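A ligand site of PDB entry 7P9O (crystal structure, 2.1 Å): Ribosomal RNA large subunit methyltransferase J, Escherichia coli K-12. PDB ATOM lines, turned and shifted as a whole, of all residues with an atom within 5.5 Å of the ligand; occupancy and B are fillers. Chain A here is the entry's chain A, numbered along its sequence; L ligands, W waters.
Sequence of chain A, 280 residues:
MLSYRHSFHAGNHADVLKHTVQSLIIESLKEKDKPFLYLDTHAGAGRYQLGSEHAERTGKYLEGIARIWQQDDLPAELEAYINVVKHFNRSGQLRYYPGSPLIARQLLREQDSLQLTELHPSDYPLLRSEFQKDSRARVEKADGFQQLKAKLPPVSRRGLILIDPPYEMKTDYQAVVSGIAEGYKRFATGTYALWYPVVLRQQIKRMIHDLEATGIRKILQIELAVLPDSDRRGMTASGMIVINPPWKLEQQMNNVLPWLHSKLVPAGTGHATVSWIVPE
The backbone carbonyl oxygen (O) of Ala 142 lies close to a nitrogen (N6) of the ligand.
Thr 41 touches the ligand (O to C13, 3.7 Å).
Ala 43 touches the ligand (O to C2, 3.5 Å).
CA of Gly 44 touches O4 of the ligand, 3.7 Å away.
Tyr 48 touches the ligand (CE2 to O2, 3.9 Å).
Gly 99 touches the ligand (CA to O2, 3.3 Å).
His 120 touches the ligand.
CG of Pro 166 touches C10 of the ligand (3.7 Å).
The nearest printed residue that does not touch the ligand is Phe 145 (4.04 Å).
Water W2 bridges N2 of the ligand and O of Asp 164.
Water W1 lies within hydrogen-bond range of the backbone carbonyl oxygen (O) of Ala 43 (2.9 Å), the backbone NH (N) of Ala 45 (3.2 Å), the side-chain hydroxyl (OH) of Tyr 48 (3.2 Å) and an oxygen (O2) of the ligand (3.2 Å).
The side-chain carboxylate of Asp 164 lies within salt-bridge range of the side-chain amino group of Lys 18, at 2.9 Å.
OE2 of Glu 118 sits at hydrogen-bond distance from N of His 120 (2.9 Å).
The side-chain carboxylate of Glu 118 is in hydrogen-bond range of the backbone NH of Gly 44, at 2.7 Å.
The backbone NH of Ser 100 sits at hydrogen-bond distance from a ring nitrogen (NE2) of His 19 (3.0 Å).
The side-chain carboxylate (OD2) of Asp 40 is in hydrogen-bond range of the side-chain hydroxyl (OG) of Ser 100, at 2.6 Å.
NZ of Lys 18 lies within salt-bridge range of OD1 of Asp 15 (3.1 Å).
N of Ala 43 sits at hydrogen-bond distance from O of Thr 117, 2.9 Å away.
OG1 of Thr 117 sits at hydrogen-bond distance from O of Thr 41, 2.5 Å away.
The side-chain carboxylate of Asp 164 lies within salt-bridge range of a nitrogen (N1) of the ligand (2.8 Å).
OE1 of Glu 118 lies within hydrogen-bond range of O4 of the ligand, at 2.8 Å.
An oxygen (O1) of the ligand lies within hydrogen-bond range of the backbone NH (N) of Ser 100 (3.1 Å).
OG of Ser 100 sits at hydrogen-bond distance from N1 of the ligand.
The side-chain carboxylate (OD2) of Asp 123 lies within hydrogen-bond range of an oxygen (O4) of the ligand (2.9 Å).
The backbone carbonyl oxygen (O) of His 42 lies within hydrogen-bond range of a nitrogen (N1) of the ligand (2.9 Å).
NE2 of His 19 lies within hydrogen-bond range of O1 of the ligand (2.9 Å).
The side-chain carboxylate (OD1) of Asp 143 sits at hydrogen-bond distance from a nitrogen (N7) of the ligand (3.0 Å).
N of Gly 144 is in hydrogen-bond range of N6 of the ligand (3.0 Å).
The backbone NH (N) of Leu 119 sits at hydrogen-bond distance from a nitrogen (N5) of the ligand (3.3 Å).
NZ of Lys 18 is in salt-bridge range of O1 of the ligand (3.6 Å).
The side-chain carboxylate (OD1) of Asp 40 is in salt-bridge range of a nitrogen (N1) of the ligand (3.97 Å).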
ATOM      1  N   ASP A  15      -3.019  23.438  -7.999  1.00  0.00           N
ATOM      2  CA  ASP A  15      -2.156  22.708  -7.047  1.00  0.00           C
ATOM      3  C   ASP A  15      -2.972  22.202  -5.832  1.00  0.00           C
ATOM      4  O   ASP A  15      -2.854  21.056  -5.500  1.00  0.00           O
ATOM      5  CB  ASP A  15      -0.955  23.591  -6.713  1.00  0.00           C
ATOM      6  CG  ASP A  15       0.097  23.693  -7.808  1.00  0.00           C
ATOM      7  OD1 ASP A  15      -0.047  23.040  -8.842  1.00  0.00           O
ATOM      8  OD2 ASP A  15       1.049  24.434  -7.602  1.00  0.00           O
ATOM      9  N   LYS A  18      -5.036  19.145  -7.127  1.00  0.00           N
ATOM     10  CA  LYS A  18      -4.156  17.994  -7.499  1.00  0.00           C
ATOM     11  C   LYS A  18      -3.464  17.419  -6.261  1.00  0.00           C
ATOM     12  O   LYS A  18      -3.494  16.219  -6.096  1.00  0.00           O
ATOM     13  CB  LYS A  18      -3.126  18.487  -8.521  1.00  0.00           C
ATOM     14  CG  LYS A  18      -1.980  17.558  -8.845  1.00  0.00           C
ATOM     15  CD  LYS A  18      -0.973  18.208  -9.760  1.00  0.00           C
ATOM     16  CE  LYS A  18      -0.184  19.320  -9.108  1.00  0.00           C
ATOM     17  NZ  LYS A  18       0.304  20.288 -10.114  1.00  0.00           N
ATOM     18  N   HIS A  19      -2.944  18.290  -5.408  1.00  0.00           N
ATOM     19  CA  HIS A  19      -2.226  17.870  -4.181  1.00  0.00           C
ATOM     20  C   HIS A  19      -3.222  17.355  -3.117  1.00  0.00           C
ATOM     21  O   HIS A  19      -2.860  16.408  -2.428  1.00  0.00           O
ATOM     22  CB  HIS A  19      -1.245  18.944  -3.771  1.00  0.00           C
ATOM     23  CG  HIS A  19      -0.122  19.118  -4.728  1.00  0.00           C
ATOM     24  ND1 HIS A  19       0.425  20.336  -4.990  1.00  0.00           N
ATOM     25  CD2 HIS A  19       0.530  18.227  -5.493  1.00  0.00           C
ATOM     26  CE1 HIS A  19       1.392  20.193  -5.874  1.00  0.00           C
ATOM     27  NE2 HIS A  19       1.466  18.921  -6.192  1.00  0.00           N
ATOM     28  N   ASP A  40       5.864   9.499 -10.320  1.00  0.00           N
ATOM     29  CA  ASP A  40       5.554  10.901 -10.631  1.00  0.00           C
ATOM     30  C   ASP A  40       6.214  11.197 -11.975  1.00  0.00           C
ATOM     31  O   ASP A  40       7.430  11.403 -12.010  1.00  0.00           O
ATOM     32  CB  ASP A  40       6.083  11.823  -9.531  1.00  0.00           C
ATOM     33  CG  ASP A  40       5.505  13.221  -9.593  1.00  0.00           C
ATOM     34  OD1 ASP A  40       5.303  13.746 -10.693  1.00  0.00           O
ATOM     35  OD2 ASP A  40       5.277  13.811  -8.521  1.00  0.00           O
ATOM     36  N   THR A  41       5.432  11.190 -13.061  1.00  0.00           N
ATOM     37  CA  THR A  41       6.021  11.217 -14.404  1.00  0.00           C
ATOM     38  C   THR A  41       6.632  12.573 -14.724  1.00  0.00           C
ATOM     39  O   THR A  41       7.655  12.637 -15.417  1.00  0.00           O
ATOM     40  CB  THR A  41       4.976  10.855 -15.455  1.00  0.00           C
ATOM     41  OG1 THR A  41       3.951  11.868 -15.526  1.00  0.00           O
ATOM     42  CG2 THR A  41       4.340   9.499 -15.148  1.00  0.00           C
ATOM     43  N   HIS A  42       6.031  13.635 -14.252  1.00  0.00           N
ATOM     44  CA  HIS A  42       6.471  15.014 -14.524  1.00  0.00           C
ATOM     45  C   HIS A  42       6.588  15.581 -13.127  1.00  0.00           C
ATOM     46  O   HIS A  42       5.586  16.144 -12.669  1.00  0.00           O
ATOM     47  CB  HIS A  42       5.432  15.733 -15.388  1.00  0.00           C
ATOM     48  CG  HIS A  42       5.320  15.339 -16.818  1.00  0.00           C
ATOM     49  ND1 HIS A  42       4.671  14.197 -17.224  1.00  0.00           N
ATOM     50  CD2 HIS A  42       5.723  15.956 -17.947  1.00  0.00           C
ATOM     51  CE1 HIS A  42       4.641  14.149 -18.540  1.00  0.00           C
ATOM     52  NE2 HIS A  42       5.280  15.215 -19.004  1.00  0.00           N
ATOM     53  N   ALA A  43       7.754  15.498 -12.505  1.00  0.00           N
ATOM     54  CA  ALA A  43       7.890  15.758 -11.085  1.00  0.00           C
ATOM     55  C   ALA A  43       8.141  17.219 -10.743  1.00  0.00           C
ATOM     56  O   ALA A  43       7.977  17.605  -9.573  1.00  0.00           O
ATOM     57  CB  ALA A  43       9.017  14.893 -10.496  1.00  0.00           C
ATOM     58  N   GLY A  44       8.546  18.036 -11.701  1.00  0.00           N
ATOM     59  CA  GLY A  44       8.858  19.415 -11.363  1.00  0.00           C
ATOM     60  C   GLY A  44      10.138  19.517 -10.556  1.00  0.00           C
ATOM     61  O   GLY A  44      10.990  18.618 -10.527  1.00  0.00           O
ATOM     62  N   ALA A  45      10.261  20.641  -9.857  1.00  0.00           N
ATOM     63  CA  ALA A  45      11.486  20.967  -9.150  1.00  0.00           C
ATOM     64  C   ALA A  45      11.558  20.387  -7.748  1.00  0.00           C
ATOM     65  O   ALA A  45      12.655  20.210  -7.219  1.00  0.00           O
ATOM     66  CB  ALA A  45      11.638  22.495  -9.091  1.00  0.00           C
ATOM     67  N   TYR A  48       8.830  25.182  -4.246  1.00  0.00           N
ATOM     68  CA  TYR A  48       8.836  26.454  -4.946  1.00  0.00           C
ATOM     69  C   TYR A  48       8.854  27.559  -3.914  1.00  0.00           C
ATOM     70  O   TYR A  48       8.031  27.580  -2.995  1.00  0.00           O
ATOM     71  CB  TYR A  48       7.623  26.582  -5.877  1.00  0.00           C
ATOM     72  CG  TYR A  48       7.684  25.517  -6.941  1.00  0.00           C
ATOM     73  CD1 TYR A  48       8.521  25.648  -8.043  1.00  0.00           C
ATOM     74  CD2 TYR A  48       6.947  24.331  -6.807  1.00  0.00           C
ATOM     75  CE1 TYR A  48       8.593  24.674  -9.010  1.00  0.00           C
ATOM     76  CE2 TYR A  48       7.031  23.344  -7.750  1.00  0.00           C
ATOM     77  CZ  TYR A  48       7.856  23.524  -8.856  1.00  0.00           C
ATOM     78  OH  TYR A  48       7.921  22.550  -9.808  1.00  0.00           O
ATOM     79  N   PRO A  98       5.195  22.998  -1.413  1.00  0.00           N
ATOM     80  CA  PRO A  98       5.707  21.684  -1.848  1.00  0.00           C
ATOM     81  C   PRO A  98       4.994  21.145  -3.095  1.00  0.00           C
ATOM     82  O   PRO A  98       3.763  21.043  -3.136  1.00  0.00           O
ATOM     83  CB  PRO A  98       5.460  20.776  -0.637  1.00  0.00           C
ATOM     84  CG  PRO A  98       4.264  21.394   0.068  1.00  0.00           C
ATOM     85  CD  PRO A  98       4.335  22.911  -0.213  1.00  0.00           C
ATOM     86  N   GLY A  99       5.770  20.780  -4.087  1.00  0.00           N
ATOM     87  CA  GLY A  99       5.230  20.063  -5.215  1.00  0.00           C
ATOM     88  C   GLY A  99       4.979  18.590  -4.917  1.00  0.00           C
ATOM     89  O   GLY A  99       5.368  18.062  -3.881  1.00  0.00           O
ATOM     90  N   SER A 100       4.294  17.936  -5.839  1.00  0.00           N
ATOM     91  CA  SER A 100       3.949  16.508  -5.816  1.00  0.00           C
ATOM     92  C   SER A 100       5.050  15.615  -5.226  1.00  0.00           C
ATOM     93  O   SER A 100       4.743  14.694  -4.447  1.00  0.00           O
ATOM     94  CB  SER A 100       3.640  16.027  -7.233  1.00  0.00           C
ATOM     95  OG  SER A 100       4.716  16.282  -8.122  1.00  0.00           O
ATOM     96  N   PRO A 101       6.333  15.831  -5.549  1.00  0.00           N
ATOM     97  CA  PRO A 101       7.362  14.900  -5.039  1.00  0.00           C
ATOM     98  C   PRO A 101       7.563  14.998  -3.552  1.00  0.00           C
ATOM     99  O   PRO A 101       7.903  13.987  -2.919  1.00  0.00           O
ATOM    100  CB  PRO A 101       8.633  15.304  -5.800  1.00  0.00           C
ATOM    101  CG  PRO A 101       8.156  16.086  -6.983  1.00  0.00           C
ATOM    102  CD  PRO A 101       6.915  16.796  -6.490  1.00  0.00           C
ATOM    103  N   THR A 117      10.596  11.571 -12.437  1.00  0.00           N
ATOM    104  CA  THR A 117      11.237  12.002 -13.666  1.00  0.00           C
ATOM    105  C   THR A 117      10.905  13.465 -13.910  1.00  0.00           C
ATOM    106  O   THR A 117       9.744  13.880 -13.800  1.00  0.00           O
ATOM    107  CB  THR A 117      10.773  11.167 -14.849  1.00  0.00           C
ATOM    108  OG1 THR A 117       9.375  10.920 -14.697  1.00  0.00           O
ATOM    109  CG2 THR A 117      11.515   9.813 -14.849  1.00  0.00           C
ATOM    110  N   GLU A 118      11.933  14.234 -14.256  1.00  0.00           N
ATOM    111  CA  GLU A 118      11.849  15.653 -14.562  1.00  0.00           C
ATOM    112  C   GLU A 118      12.839  15.908 -15.697  1.00  0.00           C
ATOM    113  O   GLU A 118      14.006  15.527 -15.586  1.00  0.00           O
ATOM    114  CB  GLU A 118      12.179  16.514 -13.327  1.00  0.00           C
ATOM    115  CG  GLU A 118      12.292  18.028 -13.530  1.00  0.00           C
ATOM    116  CD  GLU A 118      11.153  18.605 -14.342  1.00  0.00           C
ATOM    117  OE1 GLU A 118      10.002  18.656 -13.868  1.00  0.00           O
ATOM    118  OE2 GLU A 118      11.401  19.041 -15.471  1.00  0.00           O
ATOM    119  N   LEU A 119      12.360  16.492 -16.788  1.00  0.00           N
ATOM    120  CA  LEU A 119      13.140  16.549 -18.020  1.00  0.00           C
ATOM    121  C   LEU A 119      13.888  17.859 -18.204  1.00  0.00           C
ATOM    122  O   LEU A 119      14.916  17.872 -18.876  1.00  0.00           O
ATOM    123  CB  LEU A 119      12.214  16.307 -19.230  1.00  0.00           C
ATOM    124  CG  LEU A 119      12.733  15.957 -20.632  1.00  0.00           C
ATOM    125  CD1 LEU A 119      13.650  14.767 -20.609  1.00  0.00           C
ATOM    126  CD2 LEU A 119      11.583  15.667 -21.559  1.00  0.00           C
ATOM    127  N   HIS A 120      13.396  18.980 -17.595  1.00  0.00           N
ATOM    128  CA  HIS A 120      13.934  20.308 -17.880  1.00  0.00           C
ATOM    129  C   HIS A 120      15.178  20.578 -17.036  1.00  0.00           C
ATOM    130  O   HIS A 120      15.183  20.323 -15.834  1.00  0.00           O
ATOM    131  CB  HIS A 120      12.894  21.396 -17.618  1.00  0.00           C
ATOM    132  CG  HIS A 120      13.318  22.748 -18.122  1.00  0.00           C
ATOM    133  ND1 HIS A 120      14.296  23.506 -17.494  1.00  0.00           N
ATOM    134  CD2 HIS A 120      12.892  23.489 -19.166  1.00  0.00           C
ATOM    135  CE1 HIS A 120      14.453  24.639 -18.143  1.00  0.00           C
ATOM    136  NE2 HIS A 120      13.611  24.664 -19.167  1.00  0.00           N
ATOM    137  N   ASP A 123      14.925  22.618 -13.526  1.00  0.00           N
ATOM    138  CA  ASP A 123      14.332  21.963 -12.361  1.00  0.00           C
ATOM    139  C   ASP A 123      15.092  20.697 -11.966  1.00  0.00           C
ATOM    140  O   ASP A 123      15.372  20.478 -10.779  1.00  0.00           O
ATOM    141  CB  ASP A 123      12.870  21.622 -12.638  1.00  0.00           C
ATOM    142  CG  ASP A 123      12.037  22.835 -12.998  1.00  0.00           C
ATOM    143  OD1 ASP A 123      12.383  23.958 -12.584  1.00  0.00           O
ATOM    144  OD2 ASP A 123      10.997  22.639 -13.673  1.00  0.00           O
ATOM    145  N   ALA A 142      14.334  12.252 -17.614  1.00  0.00           N
ATOM    146  CA  ALA A 142      13.834  11.393 -18.674  1.00  0.00           C
ATOM    147  C   ALA A 142      12.419  11.777 -19.051  1.00  0.00           C
ATOM    148  O   ALA A 142      11.718  12.491 -18.326  1.00  0.00           O
ATOM    149  CB  ALA A 142      13.883   9.916 -18.265  1.00  0.00           C
ATOM    150  N   ASP A 143      11.976  11.279 -20.206  1.00  0.00           N
ATOM    151  CA  ASP A 143      10.624  11.525 -20.658  1.00  0.00           C
ATOM    152  C   ASP A 143       9.626  10.774 -19.785  1.00  0.00           C
ATOM    153  O   ASP A 143       9.598   9.541 -19.773  1.00  0.00           O
ATOM    154  CB  ASP A 143      10.469  11.103 -22.116  1.00  0.00           C
ATOM    155  CG  ASP A 143       9.047  11.207 -22.578  1.00  0.00           C
ATOM    156  OD1 ASP A 143       8.290  11.918 -21.885  1.00  0.00           O
ATOM    157  OD2 ASP A 143       8.684  10.598 -23.613  1.00  0.00           O
ATOM    158  N   GLY A 144       8.781  11.527 -19.070  1.00  0.00           N
ATOM    159  CA  GLY A 144       7.883  10.911 -18.101  1.00  0.00           C
ATOM    160  C   GLY A 144       6.968   9.861 -18.698  1.00  0.00           C
ATOM    161  O   GLY A 144       6.767   8.808 -18.101  1.00  0.00           O
ATOM    162  N   PHE A 145       6.398  10.139 -19.882  1.00  0.00           N
ATOM    163  CA  PHE A 145       5.537   9.154 -20.522  1.00  0.00           C
ATOM    164  C   PHE A 145       6.261   7.827 -20.728  1.00  0.00           C
ATOM    165  O   PHE A 145       5.650   6.757 -20.635  1.00  0.00           O
ATOM    166  CB  PHE A 145       5.030   9.676 -21.870  1.00  0.00           C
ATOM    167  CG  PHE A 145       4.425  11.046 -21.812  1.00  0.00           C
ATOM    168  CD1 PHE A 145       3.114  11.211 -21.374  1.00  0.00           C
ATOM    169  CD2 PHE A 145       5.147  12.158 -22.216  1.00  0.00           C
ATOM    170  CE1 PHE A 145       2.545  12.474 -21.332  1.00  0.00           C
ATOM    171  CE2 PHE A 145       4.599  13.417 -22.170  1.00  0.00           C
ATOM    172  CZ  PHE A 145       3.297  13.577 -21.734  1.00  0.00           C
ATOM    173  N   LEU A 162       1.165   9.371 -10.800  1.00  0.00           N
ATOM    174  CA  LEU A 162       0.697  10.737 -10.996  1.00  0.00           C
ATOM    175  C   LEU A 162       1.255  11.254 -12.308  1.00  0.00           C
ATOM    176  O   LEU A 162       2.469  11.244 -12.520  1.00  0.00           O
ATOM    177  CB  LEU A 162       1.137  11.635  -9.842  1.00  0.00           C
ATOM    178  CG  LEU A 162       0.781  13.120 -10.001  1.00  0.00           C
ATOM    179  CD1 LEU A 162      -0.645  13.405  -9.527  1.00  0.00           C
ATOM    180  CD2 LEU A 162       1.784  13.989  -9.257  1.00  0.00           C
ATOM    181  N   ASP A 164       1.235  14.569 -14.511  1.00  0.00           N
ATOM    182  CA  ASP A 164       0.940  15.987 -14.309  1.00  0.00           C
ATOM    183  C   ASP A 164       1.706  16.832 -15.331  1.00  0.00           C
ATOM    184  O   ASP A 164       2.591  17.619 -14.984  1.00  0.00           O
ATOM    185  CB  ASP A 164       1.267  16.377 -12.872  1.00  0.00           C
ATOM    186  CG  ASP A 164       0.986  17.841 -12.567  1.00  0.00           C
ATOM    187  OD1 ASP A 164       0.027  18.412 -13.113  1.00  0.00           O
ATOM    188  OD2 ASP A 164       1.751  18.419 -11.768  1.00  0.00           O
ATOM    189  N   PRO A 165       1.374  16.682 -16.613  1.00  0.00           N
ATOM    190  CA  PRO A 165       2.136  17.373 -17.670  1.00  0.00           C
ATOM    191  C   PRO A 165       1.717  18.833 -17.765  1.00  0.00           C
ATOM    192  O   PRO A 165       0.628  19.209 -17.301  1.00  0.00           O
ATOM    193  CB  PRO A 165       1.767  16.595 -18.948  1.00  0.00           C
ATOM    194  CG  PRO A 165       0.593  15.726 -18.584  1.00  0.00           C
ATOM    195  CD  PRO A 165       0.188  16.016 -17.160  1.00  0.00           C
ATOM    196  N   PRO A 166       2.565  19.685 -18.350  1.00  0.00           N
ATOM    197  CA  PRO A 166       2.251  21.122 -18.387  1.00  0.00           C
ATOM    198  C   PRO A 166       1.333  21.503 -19.525  1.00  0.00           C
ATOM    199  O   PRO A 166       0.850  22.644 -19.540  1.00  0.00           O
ATOM    200  CB  PRO A 166       3.633  21.770 -18.547  1.00  0.00           C
ATOM    201  CG  PRO A 166       4.554  20.658 -19.052  1.00  0.00           C
ATOM    202  CD  PRO A 166       3.764  19.380 -19.138  1.00  0.00           C
HETATM  203  O1  LIG L   1       3.142  18.794  -8.554  1.00  0.00           O
HETATM  204  C1  LIG L   1       4.137  19.355  -9.041  1.00  0.00           C
HETATM  205  O2  LIG L   1       4.637  20.385  -8.478  1.00  0.00           O
HETATM  206  C2  LIG L   1       4.728  18.796 -10.310  1.00  0.00           C
HETATM  207  N1  LIG L   1       4.116  17.529 -10.605  1.00  0.00           N
HETATM  208  C3  LIG L   1       4.495  19.827 -11.494  1.00  0.00           C
HETATM  209  C4  LIG L   1       4.825  19.230 -12.862  1.00  0.00           C
HETATM  210  N2  LIG L   1       4.874  20.326 -13.910  1.00  0.00           N
HETATM  211  C5  LIG L   1       5.548  19.760 -15.107  1.00  0.00           C
HETATM  212  C6  LIG L   1       7.075  19.720 -14.843  1.00  0.00           C
HETATM  213  O3  LIG L   1       7.671  18.450 -15.482  1.00  0.00           O
HETATM  214  C7  LIG L   1       7.705  20.732 -15.422  1.00  0.00           C
HETATM  215  O4  LIG L   1       8.832  21.063 -14.659  1.00  0.00           O
HETATM  216  C8  LIG L   1       8.156  20.216 -16.872  1.00  0.00           C
HETATM  217  O5  LIG L   1       9.358  20.918 -17.258  1.00  0.00           O
HETATM  218  C9  LIG L   1       8.457  18.928 -16.717  1.00  0.00           C
HETATM  219  N3  LIG L   1       8.230  18.277 -18.072  1.00  0.00           N
HETATM  220  C10 LIG L   1       7.700  18.699 -19.196  1.00  0.00           C
HETATM  221  N4  LIG L   1       7.706  17.717 -20.093  1.00  0.00           N
HETATM  222  C11 LIG L   1       8.273  16.638 -19.512  1.00  0.00           C
HETATM  223  C12 LIG L   1       8.589  17.000 -18.247  1.00  0.00           C
HETATM  224  N5  LIG L   1       9.159  16.118 -17.399  1.00  0.00           N
HETATM  225  C13 LIG L   1       9.425  14.890 -17.804  1.00  0.00           C
HETATM  226  N6  LIG L   1       9.142  14.493 -19.009  1.00  0.00           N
HETATM  227  C14 LIG L   1       8.570  15.318 -19.890  1.00  0.00           C
HETATM  228  N7  LIG L   1       8.258  14.831 -21.220  1.00  0.00           N
HETATM  229  O   HOH W   1       7.785  19.940  -7.924  1.00  0.00           O
HETATM  230  O   HOH W   2       2.159  20.882 -14.312  1.00  0.00           O
